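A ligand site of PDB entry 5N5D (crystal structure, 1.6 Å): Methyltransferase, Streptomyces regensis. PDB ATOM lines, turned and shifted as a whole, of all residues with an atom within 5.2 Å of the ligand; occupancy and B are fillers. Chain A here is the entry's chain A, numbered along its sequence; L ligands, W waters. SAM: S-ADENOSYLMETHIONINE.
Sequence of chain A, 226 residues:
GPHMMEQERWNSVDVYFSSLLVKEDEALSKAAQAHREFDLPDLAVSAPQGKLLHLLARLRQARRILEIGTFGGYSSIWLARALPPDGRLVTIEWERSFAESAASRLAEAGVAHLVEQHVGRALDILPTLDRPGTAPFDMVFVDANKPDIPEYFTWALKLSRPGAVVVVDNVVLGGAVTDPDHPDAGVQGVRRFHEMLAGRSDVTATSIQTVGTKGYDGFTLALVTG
Water W3 lies within hydrogen-bond range of the side-chain hydroxyl of Tyr 152 (2.9 Å), a nitrogen (N6) of the ligand (3.0 Å) and the backbone NH of Ala 122 (3.3 Å).
Water W4 lies within hydrogen-bond range of the side-chain amide nitrogen of Asn 145 and a nitrogen (N6) of the ligand.
Residues that only touch the ligand: Leu 43 (3.3 Å), Ala 44 (3.4 Å), Thr 70 (3.7 Å), Tyr 74 (3.4 Å), Phe 98 (3.6 Å), Gly 120 (3.5 Å), Arg 121 (3.8 Å), Phe 141 (3.9 Å) and Ala 144 (3.5 Å).
Hydrophobic or aromatic side chains that line the ligand: Leu 43, Ala 44, Val 45, Phe 71, Tyr 74, Trp 94, Phe 98, Ala 122, Phe 141 and Ala 144.
Within 4 Å of the ligand: Leu 43, Ala 44, Val 45, Gly 69, Thr 70, Phe 71, Tyr 74, Ser 75, Glu 93, Trp 94, Phe 98, Gly 120, Arg 121, Ala 122, Phe 141, Asp 143, Ala 144, Asn 145 and Tyr 152.
Along chain A the residues within 4 Å of the ligand span positions 43 to 152.
The nearest printed residue that does not touch the ligand is Glu 67 (4.03 Å).
OG of Ser 75 sits at hydrogen-bond distance from OE2 of Glu 67 (2.6 Å).
The side-chain hydroxyl (OH) of Tyr 152 is in hydrogen-bond range of the side-chain amide oxygen (OD1) of Asn 145, at 2.6 Å.
O of Glu 93 sits at hydrogen-bond distance from N of Gly 120 (2.9 Å).
The backbone NH (N) of Gly 69 sits at hydrogen-bond distance from the backbone carbonyl oxygen (O) of Ile 92 (2.8 Å).
The backbone NH (N) of Phe 71 is in hydrogen-bond range of the side-chain carboxylate (OE1) of Glu 93 (2.9 Å).
The backbone NH (N) of Thr 70 lies within hydrogen-bond range of the side-chain carboxylate (OE1) of Glu 93, 3.5 Å away.
The side-chain amide nitrogen (ND2) of Asn 145 lies within hydrogen-bond range of the side-chain carboxylate (OD2) of Asp 148.
The backbone carbonyl oxygen of Ile 92 sits at hydrogen-bond distance from the backbone NH of Thr 70.
The side-chain carboxylate (OE2) of Glu 93 sits at hydrogen-bond distance from an oxygen (O2') of the ligand (2.6 Å).
N of Ala 122 sits at hydrogen-bond distance from N1 of the ligand (3.0 Å).
A nitrogen (N6) of the ligand lies within hydrogen-bond range of the side-chain amide oxygen (OD1) of Asn 145 (3.3 Å).
OH of Tyr 152 is in hydrogen-bond range of N6 of the ligand (3.4 Å).
O3' of the ligand lies close to N of Phe 71, 3.5 Å away.
The side-chain hydroxyl of Ser 75 is in hydrogen-bond range of a nitrogen (N) of the ligand (2.8 Å).
OD2 of Asp 143 lies within salt-bridge range of N of the ligand, 2.8 Å away.
O of Gly 69 lies within hydrogen-bond range of N of the ligand, at 2.8 Å.
An oxygen (O) of the ligand lies within hydrogen-bond range of the backbone NH (N) of Val 45 (2.9 Å).
The backbone NH (N) of Ser 75 is in hydrogen-bond range of an oxygen (OXT) of the ligand (3.1 Å).
N of Trp 94 lies within hydrogen-bond range of N3 of the ligand (3.1 Å).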
ATOM      1  N   LEU A  43     -10.687  29.005  20.328  1.00  0.00           N
ATOM      2  CA  LEU A  43     -10.241  28.484  19.054  1.00  0.00           C
ATOM      3  C   LEU A  43      -9.905  29.566  18.034  1.00  0.00           C
ATOM      4  O   LEU A  43      -9.390  29.250  16.959  1.00  0.00           O
ATOM      5  CB  LEU A  43     -11.307  27.578  18.454  1.00  0.00           C
ATOM      6  CG  LEU A  43     -11.809  26.439  19.329  1.00  0.00           C
ATOM      7  CD1 LEU A  43     -12.864  25.633  18.584  1.00  0.00           C
ATOM      8  CD2 LEU A  43     -10.649  25.542  19.765  1.00  0.00           C
ATOM      9  N   ALA A  44     -10.177  30.834  18.353  1.00  0.00           N
ATOM     10  CA  ALA A  44      -9.994  31.906  17.386  1.00  0.00           C
ATOM     11  C   ALA A  44      -8.538  32.331  17.301  1.00  0.00           C
ATOM     12  O   ALA A  44      -7.778  32.223  18.266  1.00  0.00           O
ATOM     13  CB  ALA A  44     -10.851  33.110  17.755  1.00  0.00           C
ATOM     14  N   VAL A  45      -8.150  32.825  16.126  1.00  0.00           N
ATOM     15  CA  VAL A  45      -6.868  33.515  16.015  1.00  0.00           C
ATOM     16  C   VAL A  45      -6.840  34.634  17.055  1.00  0.00           C
ATOM     17  O   VAL A  45      -7.882  35.196  17.419  1.00  0.00           O
ATOM     18  CB  VAL A  45      -6.631  34.086  14.602  1.00  0.00           C
ATOM     19  CG1 VAL A  45      -6.526  32.947  13.579  1.00  0.00           C
ATOM     20  CG2 VAL A  45      -7.731  35.059  14.216  1.00  0.00           C
ATOM     21  N   GLU A  67     -12.621  31.114   3.335  1.00  0.00           N
ATOM     22  CA  GLU A  67     -12.253  30.703   4.687  1.00  0.00           C
ATOM     23  C   GLU A  67     -12.904  29.371   5.004  1.00  0.00           C
ATOM     24  O   GLU A  67     -14.109  29.204   4.836  1.00  0.00           O
ATOM     25  CB  GLU A  67     -12.695  31.755   5.715  1.00  0.00           C
ATOM     26  CG  GLU A  67     -12.491  31.350   7.166  1.00  0.00           C
ATOM     27  CD  GLU A  67     -12.895  32.446   8.117  1.00  0.00           C
ATOM     28  OE1 GLU A  67     -14.091  32.785   8.162  1.00  0.00           O
ATOM     29  OE2 GLU A  67     -11.996  32.983   8.808  1.00  0.00           O
ATOM     30  N   GLY A  69     -13.598  27.186   8.068  1.00  0.00           N
ATOM     31  CA  GLY A  69     -13.630  27.189   9.526  1.00  0.00           C
ATOM     32  C   GLY A  69     -14.018  28.533  10.132  1.00  0.00           C
ATOM     33  O   GLY A  69     -13.162  29.211  10.713  1.00  0.00           O
ATOM     34  N   THR A  70     -15.298  28.895  10.035  1.00  0.00           N
ATOM     35  CA  THR A  70     -15.770  30.191  10.530  1.00  0.00           C
ATOM     36  C   THR A  70     -15.663  30.294  12.045  1.00  0.00           C
ATOM     37  O   THR A  70     -15.322  31.365  12.572  1.00  0.00           O
ATOM     38  CB  THR A  70     -17.231  30.404  10.138  1.00  0.00           C
ATOM     39  OG1 THR A  70     -17.447  29.989   8.791  1.00  0.00           O
ATOM     40  CG2 THR A  70     -17.617  31.872  10.301  1.00  0.00           C
ATOM     41  N   PHE A  71     -15.985  29.211  12.759  1.00  0.00           N
ATOM     42  CA  PHE A  71     -16.248  29.256  14.188  1.00  0.00           C
ATOM     43  C   PHE A  71     -17.151  30.446  14.501  1.00  0.00           C
ATOM     44  O   PHE A  71     -18.267  30.516  13.966  1.00  0.00           O
ATOM     45  CB  PHE A  71     -14.946  29.284  15.000  1.00  0.00           C
ATOM     46  CG  PHE A  71     -15.139  29.045  16.479  1.00  0.00           C
ATOM     47  CD1 PHE A  71     -15.937  28.000  16.938  1.00  0.00           C
ATOM     48  CD2 PHE A  71     -14.508  29.856  17.414  1.00  0.00           C
ATOM     49  CE1 PHE A  71     -16.108  27.776  18.292  1.00  0.00           C
ATOM     50  CE2 PHE A  71     -14.683  29.640  18.774  1.00  0.00           C
ATOM     51  CZ  PHE A  71     -15.482  28.596  19.210  1.00  0.00           C
ATOM     52  N   GLY A  72     -16.712  31.357  15.371  1.00  0.00           N
ATOM     53  CA  GLY A  72     -17.525  32.467  15.818  1.00  0.00           C
ATOM     54  C   GLY A  72     -17.392  33.738  15.005  1.00  0.00           C
ATOM     55  O   GLY A  72     -17.980  34.761  15.366  1.00  0.00           O
ATOM     56  N   GLY A  73     -16.627  33.708  13.913  1.00  0.00           N
ATOM     57  CA  GLY A  73     -16.515  34.847  13.045  1.00  0.00           C
ATOM     58  C   GLY A  73     -15.386  35.811  13.349  1.00  0.00           C
ATOM     59  O   GLY A  73     -15.311  36.867  12.698  1.00  0.00           O
ATOM     60  N   TYR A  74     -14.505  35.480  14.293  1.00  0.00           N
ATOM     61  CA  TYR A  74     -13.445  36.421  14.658  1.00  0.00           C
ATOM     62  C   TYR A  74     -12.478  36.621  13.495  1.00  0.00           C
ATOM     63  O   TYR A  74     -12.267  37.750  13.039  1.00  0.00           O
ATOM     64  CB  TYR A  74     -12.700  35.954  15.918  1.00  0.00           C
ATOM     65  CG  TYR A  74     -11.712  36.990  16.339  1.00  0.00           C
ATOM     66  CD1 TYR A  74     -12.095  38.056  17.153  1.00  0.00           C
ATOM     67  CD2 TYR A  74     -10.404  36.958  15.878  1.00  0.00           C
ATOM     68  CE1 TYR A  74     -11.194  39.048  17.512  1.00  0.00           C
ATOM     69  CE2 TYR A  74      -9.499  37.942  16.232  1.00  0.00           C
ATOM     70  CZ  TYR A  74      -9.894  38.987  17.049  1.00  0.00           C
ATOM     71  OH  TYR A  74      -9.000  39.972  17.393  1.00  0.00           O
ATOM     72  N   SER A  75     -11.879  35.544  12.986  1.00  0.00           N
ATOM     73  CA  SER A  75     -11.039  35.687  11.809  1.00  0.00           C
ATOM     74  C   SER A  75     -11.837  36.232  10.625  1.00  0.00           C
ATOM     75  O   SER A  75     -11.305  37.010   9.827  1.00  0.00           O
ATOM     76  CB  SER A  75     -10.388  34.355  11.452  1.00  0.00           C
ATOM     77  OG  SER A  75     -11.354  33.343  11.270  1.00  0.00           O
ATOM     78  N   SER A  76     -13.116  35.868  10.541  1.00  0.00           N
ATOM     79  CA  SER A  76     -13.956  36.289   9.415  1.00  0.00           C
ATOM     80  C   SER A  76     -14.075  37.801   9.345  1.00  0.00           C
ATOM     81  O   SER A  76     -14.026  38.385   8.260  1.00  0.00           O
ATOM     82  CB  SER A  76     -15.344  35.655   9.534  1.00  0.00           C
ATOM     83  OG  SER A  76     -15.249  34.296   9.947  1.00  0.00           O
ATOM     84  N   ILE A  92     -16.967  28.784   5.527  1.00  0.00           N
ATOM     85  CA  ILE A  92     -17.596  27.486   5.730  1.00  0.00           C
ATOM     86  C   ILE A  92     -17.463  27.065   7.188  1.00  0.00           C
ATOM     87  O   ILE A  92     -16.375  27.139   7.761  1.00  0.00           O
ATOM     88  CB  ILE A  92     -16.954  26.399   4.835  1.00  0.00           C
ATOM     89  CG1 ILE A  92     -16.973  26.816   3.373  1.00  0.00           C
ATOM     90  CG2 ILE A  92     -17.665  25.064   5.048  1.00  0.00           C
ATOM     91  CD1 ILE A  92     -16.165  25.893   2.460  1.00  0.00           C
ATOM     92  N   GLU A  93     -18.554  26.558   7.748  1.00  0.00           N
ATOM     93  CA  GLU A  93     -18.582  26.087   9.134  1.00  0.00           C
ATOM     94  C   GLU A  93     -19.514  24.889   9.262  1.00  0.00           C
ATOM     95  O   GLU A  93     -20.656  24.936   8.802  1.00  0.00           O
ATOM     96  CB  GLU A  93     -19.037  27.219  10.070  1.00  0.00           C
ATOM     97  CG  GLU A  93     -19.298  26.784  11.515  1.00  0.00           C
ATOM     98  CD  GLU A  93     -18.114  26.096  12.129  1.00  0.00           C
ATOM     99  OE1 GLU A  93     -16.988  26.629  12.015  1.00  0.00           O
ATOM    100  OE2 GLU A  93     -18.285  25.012  12.728  1.00  0.00           O
ATOM    101  N   TRP A  94     -19.028  23.845   9.944  1.00  0.00           N
ATOM    102  CA  TRP A  94     -19.798  22.610  10.097  1.00  0.00           C
ATOM    103  C   TRP A  94     -20.917  22.729  11.131  1.00  0.00           C
ATOM    104  O   TRP A  94     -21.974  22.127  10.949  1.00  0.00           O
ATOM    105  CB  TRP A  94     -18.828  21.473  10.470  1.00  0.00           C
ATOM    106  CG  TRP A  94     -19.445  20.271  11.092  1.00  0.00           C
ATOM    107  CD1 TRP A  94     -19.303  19.847  12.384  1.00  0.00           C
ATOM    108  CD2 TRP A  94     -20.274  19.295  10.448  1.00  0.00           C
ATOM    109  NE1 TRP A  94     -20.003  18.693  12.588  1.00  0.00           N
ATOM    110  CE2 TRP A  94     -20.608  18.328  11.413  1.00  0.00           C
ATOM    111  CE3 TRP A  94     -20.774  19.156   9.152  1.00  0.00           C
ATOM    112  CZ2 TRP A  94     -21.427  17.232  11.119  1.00  0.00           C
ATOM    113  CZ3 TRP A  94     -21.588  18.072   8.863  1.00  0.00           C
ATOM    114  CH2 TRP A  94     -21.901  17.128   9.848  1.00  0.00           C
ATOM    115  N   GLU A  95     -20.710  23.505  12.200  1.00  0.00           N
ATOM    116  CA  GLU A  95     -21.672  23.593  13.286  1.00  0.00           C
ATOM    117  C   GLU A  95     -22.599  24.791  13.053  1.00  0.00           C
ATOM    118  O   GLU A  95     -22.147  25.932  13.048  1.00  0.00           O
ATOM    119  CB  GLU A  95     -20.949  23.730  14.624  1.00  0.00           C
ATOM    120  CG  GLU A  95     -21.822  23.537  15.851  1.00  0.00           C
ATOM    121  CD  GLU A  95     -22.358  22.126  15.961  1.00  0.00           C
ATOM    122  OE1 GLU A  95     -23.595  21.949  15.864  1.00  0.00           O
ATOM    123  OE2 GLU A  95     -21.558  21.189  16.155  1.00  0.00           O
ATOM    124  N   PHE A  98     -22.536  27.662  15.707  1.00  0.00           N
ATOM    125  CA  PHE A  98     -21.386  28.554  15.561  1.00  0.00           C
ATOM    126  C   PHE A  98     -21.617  29.529  14.414  1.00  0.00           C
ATOM    127  O   PHE A  98     -21.408  30.743  14.561  1.00  0.00           O
ATOM    128  CB  PHE A  98     -20.099  27.756  15.316  1.00  0.00           C
ATOM    129  CG  PHE A  98     -19.758  26.746  16.385  1.00  0.00           C
ATOM    130  CD1 PHE A  98     -20.475  26.668  17.581  1.00  0.00           C
ATOM    131  CD2 PHE A  98     -18.703  25.868  16.195  1.00  0.00           C
ATOM    132  CE1 PHE A  98     -20.145  25.736  18.544  1.00  0.00           C
ATOM    133  CE2 PHE A  98     -18.375  24.940  17.149  1.00  0.00           C
ATOM    134  CZ  PHE A  98     -19.090  24.860  18.331  1.00  0.00           C
ATOM    135  N   GLY A 120     -21.990  23.320   6.765  1.00  0.00           N
ATOM    136  CA  GLY A 120     -21.865  21.921   6.409  1.00  0.00           C
ATOM    137  C   GLY A 120     -20.414  21.492   6.407  1.00  0.00           C
ATOM    138  O   GLY A 120     -19.509  22.251   6.766  1.00  0.00           O
ATOM    139  N   ARG A 121     -20.202  20.241   5.995  1.00  0.00           N
ATOM    140  CA  ARG A 121     -18.866  19.692   5.885  1.00  0.00           C
ATOM    141  C   ARG A 121     -18.122  20.365   4.739  1.00  0.00           C
ATOM    142  O   ARG A 121     -18.618  20.406   3.609  1.00  0.00           O
ATOM    143  CB  ARG A 121     -18.923  18.180   5.636  1.00  0.00           C
ATOM    144  CG  ARG A 121     -18.650  17.317   6.846  1.00  0.00           C
ATOM    145  CD  ARG A 121     -18.678  15.850   6.452  1.00  0.00           C
ATOM    146  NE  ARG A 121     -17.666  15.562   5.431  1.00  0.00           N
ATOM    147  CZ  ARG A 121     -17.813  14.705   4.432  1.00  0.00           C
ATOM    148  NH1 ARG A 121     -18.950  14.037   4.267  1.00  0.00           N
ATOM    149  NH2 ARG A 121     -16.817  14.528   3.568  1.00  0.00           N
ATOM    150  N   ALA A 122     -16.926  20.879   5.027  1.00  0.00           N
ATOM    151  CA  ALA A 122     -16.201  21.648   4.018  1.00  0.00           C
ATOM    152  C   ALA A 122     -15.963  20.848   2.743  1.00  0.00           C
ATOM    153  O   ALA A 122     -16.089  21.381   1.634  1.00  0.00           O
ATOM    154  CB  ALA A 122     -14.881  22.157   4.589  1.00  0.00           C
ATOM    155  N   PHE A 141      -7.920  30.931   3.573  1.00  0.00           N
ATOM    156  CA  PHE A 141      -7.524  30.687   4.952  1.00  0.00           C
ATOM    157  C   PHE A 141      -8.121  29.348   5.381  1.00  0.00           C
ATOM    158  O   PHE A 141      -9.344  29.179   5.401  1.00  0.00           O
ATOM    159  CB  PHE A 141      -7.995  31.807   5.873  1.00  0.00           C
ATOM    160  CG  PHE A 141      -7.594  31.636   7.324  1.00  0.00           C
ATOM    161  CD1 PHE A 141      -6.317  31.214   7.668  1.00  0.00           C
ATOM    162  CD2 PHE A 141      -8.501  31.892   8.338  1.00  0.00           C
ATOM    163  CE1 PHE A 141      -5.958  31.070   9.004  1.00  0.00           C
ATOM    164  CE2 PHE A 141      -8.143  31.752   9.666  1.00  0.00           C
ATOM    165  CZ  PHE A 141      -6.869  31.335  10.001  1.00  0.00           C
ATOM    166  N   ASP A 143      -8.519  26.798   8.342  1.00  0.00           N
ATOM    167  CA  ASP A 143      -8.496  26.783   9.790  1.00  0.00           C
ATOM    168  C   ASP A 143      -9.671  25.952  10.299  1.00  0.00           C
ATOM    169  O   ASP A 143     -10.503  26.418  11.073  1.00  0.00           O
ATOM    170  CB  ASP A 143      -8.529  28.203  10.346  1.00  0.00           C
ATOM    171  CG  ASP A 143      -8.324  28.266  11.841  1.00  0.00           C
ATOM    172  OD1 ASP A 143      -7.753  27.306  12.422  1.00  0.00           O
ATOM    173  OD2 ASP A 143      -8.747  29.272  12.457  1.00  0.00           O
ATOM    174  N   ALA A 144      -9.762  24.708   9.854  1.00  0.00           N
ATOM    175  CA  ALA A 144     -10.826  23.816  10.305  1.00  0.00           C
ATOM    176  C   ALA A 144     -10.198  22.581  10.932  1.00  0.00           C
ATOM    177  O   ALA A 144      -9.317  22.687  11.789  1.00  0.00           O
ATOM    178  CB  ALA A 144     -11.771  23.481   9.152  1.00  0.00           C
ATOM    179  N   ASN A 145     -10.634  21.399  10.517  1.00  0.00           N
ATOM    180  CA  ASN A 145     -10.077  20.156  11.041  1.00  0.00           C
ATOM    181  C   ASN A 145      -8.786  19.820  10.314  1.00  0.00           C
ATOM    182  O   ASN A 145      -8.640  20.060   9.113  1.00  0.00           O
ATOM    183  CB  ASN A 145     -11.090  19.033  10.891  1.00  0.00           C
ATOM    184  CG  ASN A 145     -11.523  18.816   9.468  1.00  0.00           C
ATOM    185  OD1 ASN A 145     -11.872  19.765   8.762  1.00  0.00           O
ATOM    186  ND2 ASN A 145     -11.513  17.567   9.033  1.00  0.00           N
ATOM    187  N   ASP A 148      -8.023  16.835   7.159  1.00  0.00           N
ATOM    188  CA  ASP A 148      -8.411  17.108   5.783  1.00  0.00           C
ATOM    189  C   ASP A 148      -7.588  18.234   5.142  1.00  0.00           C
ATOM    190  O   ASP A 148      -7.899  18.623   4.008  1.00  0.00           O
ATOM    191  CB  ASP A 148      -9.898  17.460   5.716  1.00  0.00           C
ATOM    192  CG  ASP A 148     -10.781  16.245   5.928  1.00  0.00           C
ATOM    193  OD1 ASP A 148     -10.367  15.120   5.585  1.00  0.00           O
ATOM    194  OD2 ASP A 148     -11.913  16.437   6.424  1.00  0.00           O
ATOM    195  N   TYR A 152      -8.085  20.092   1.611  1.00  0.00           N
ATOM    196  CA  TYR A 152      -8.383  21.512   1.578  1.00  0.00           C
ATOM    197  C   TYR A 152      -7.367  22.265   0.726  1.00  0.00           C
ATOM    198  O   TYR A 152      -7.732  23.202   0.006  1.00  0.00           O
ATOM    199  CB  TYR A 152      -8.407  22.092   2.999  1.00  0.00           C
ATOM    200  CG  TYR A 152      -9.511  21.559   3.885  1.00  0.00           C
ATOM    201  CD1 TYR A 152     -10.709  21.118   3.346  1.00  0.00           C
ATOM    202  CD2 TYR A 152      -9.353  21.502   5.267  1.00  0.00           C
ATOM    203  CE1 TYR A 152     -11.719  20.629   4.142  1.00  0.00           C
ATOM    204  CE2 TYR A 152     -10.373  21.011   6.076  1.00  0.00           C
ATOM    205  CZ  TYR A 152     -11.550  20.573   5.511  1.00  0.00           C
ATOM    206  OH  TYR A 152     -12.577  20.076   6.284  1.00  0.00           O
ATOM    207  N   ASN A 170      -2.275  26.429  12.446  1.00  0.00           N
ATOM    208  CA  ASN A 170      -2.129  25.368  13.439  1.00  0.00           C
ATOM    209  C   ASN A 170      -1.396  24.137  12.874  1.00  0.00           C
ATOM    210  O   ASN A 170      -1.836  23.001  13.041  1.00  0.00           O
ATOM    211  CB  ASN A 170      -3.494  24.984  14.011  1.00  0.00           C
ATOM    212  CG  ASN A 170      -4.243  26.181  14.573  1.00  0.00           C
ATOM    213  OD1 ASN A 170      -5.406  26.418  14.243  1.00  0.00           O
ATOM    214  ND2 ASN A 170      -3.571  26.959  15.434  1.00  0.00           N
HETATM  215  N   SAM L   1     -11.126  30.628  11.963  1.00  0.00           N
HETATM  216  CA  SAM L   1     -11.747  30.844  13.285  1.00  0.00           C
HETATM  217  C   SAM L   1     -11.139  32.106  13.972  1.00  0.00           C
HETATM  218  O   SAM L   1      -9.896  32.239  13.904  1.00  0.00           O
HETATM  219  OXT SAM L   1     -11.928  32.884  14.547  1.00  0.00           O
HETATM  220  CB  SAM L   1     -11.549  29.595  14.187  1.00  0.00           C
HETATM  221  CG  SAM L   1     -11.907  28.304  13.464  1.00  0.00           C
HETATM  222  SD  SAM L   1     -11.819  26.959  14.663  1.00  0.00           S
HETATM  223  CE  SAM L   1     -10.083  26.773  14.834  1.00  0.00           C
HETATM  224  C5' SAM L   1     -12.162  25.482  13.639  1.00  0.00           C
HETATM  225  C4' SAM L   1     -13.588  25.430  13.142  1.00  0.00           C
HETATM  226  O4' SAM L   1     -13.725  24.469  12.073  1.00  0.00           O
HETATM  227  C3' SAM L   1     -14.628  25.070  14.212  1.00  0.00           C
HETATM  228  O3' SAM L   1     -15.615  26.091  14.279  1.00  0.00           O
HETATM  229  C2' SAM L   1     -15.178  23.716  13.729  1.00  0.00           C
HETATM  230  O2' SAM L   1     -16.553  23.537  14.021  1.00  0.00           O
HETATM  231  C1' SAM L   1     -14.966  23.826  12.223  1.00  0.00           C
HETATM  232  N9  SAM L   1     -14.910  22.554  11.521  1.00  0.00           N
HETATM  233  C8  SAM L   1     -14.311  21.395  11.930  1.00  0.00           C
HETATM  234  N7  SAM L   1     -14.368  20.415  11.053  1.00  0.00           N
HETATM  235  C5  SAM L   1     -15.046  20.977   9.979  1.00  0.00           C
HETATM  236  C6  SAM L   1     -15.400  20.472   8.719  1.00  0.00           C
HETATM  237  N6  SAM L   1     -15.125  19.227   8.308  1.00  0.00           N
HETATM  238  N1  SAM L   1     -16.061  21.296   7.876  1.00  0.00           N
HETATM  239  C2  SAM L   1     -16.338  22.545   8.278  1.00  0.00           C
HETATM  240  N3  SAM L   1     -16.052  23.128   9.445  1.00  0.00           N
HETATM  241  C4  SAM L   1     -15.392  22.286  10.256  1.00  0.00           C
HETATM  242  O   HOH W   1     -14.365  17.820  12.475  1.00  0.00           O
HETATM  243  O   HOH W   2     -12.331  21.114  14.522  1.00  0.00           O
HETATM  244  O   HOH W   3     -14.744  18.385   5.506  1.00  0.00           O
HETATM  245  O   HOH W   4     -14.256  16.848  10.209  1.00  0.00           O
HETATM  246  O   HOH W   5     -14.244  32.897  15.803  1.00  0.00           O
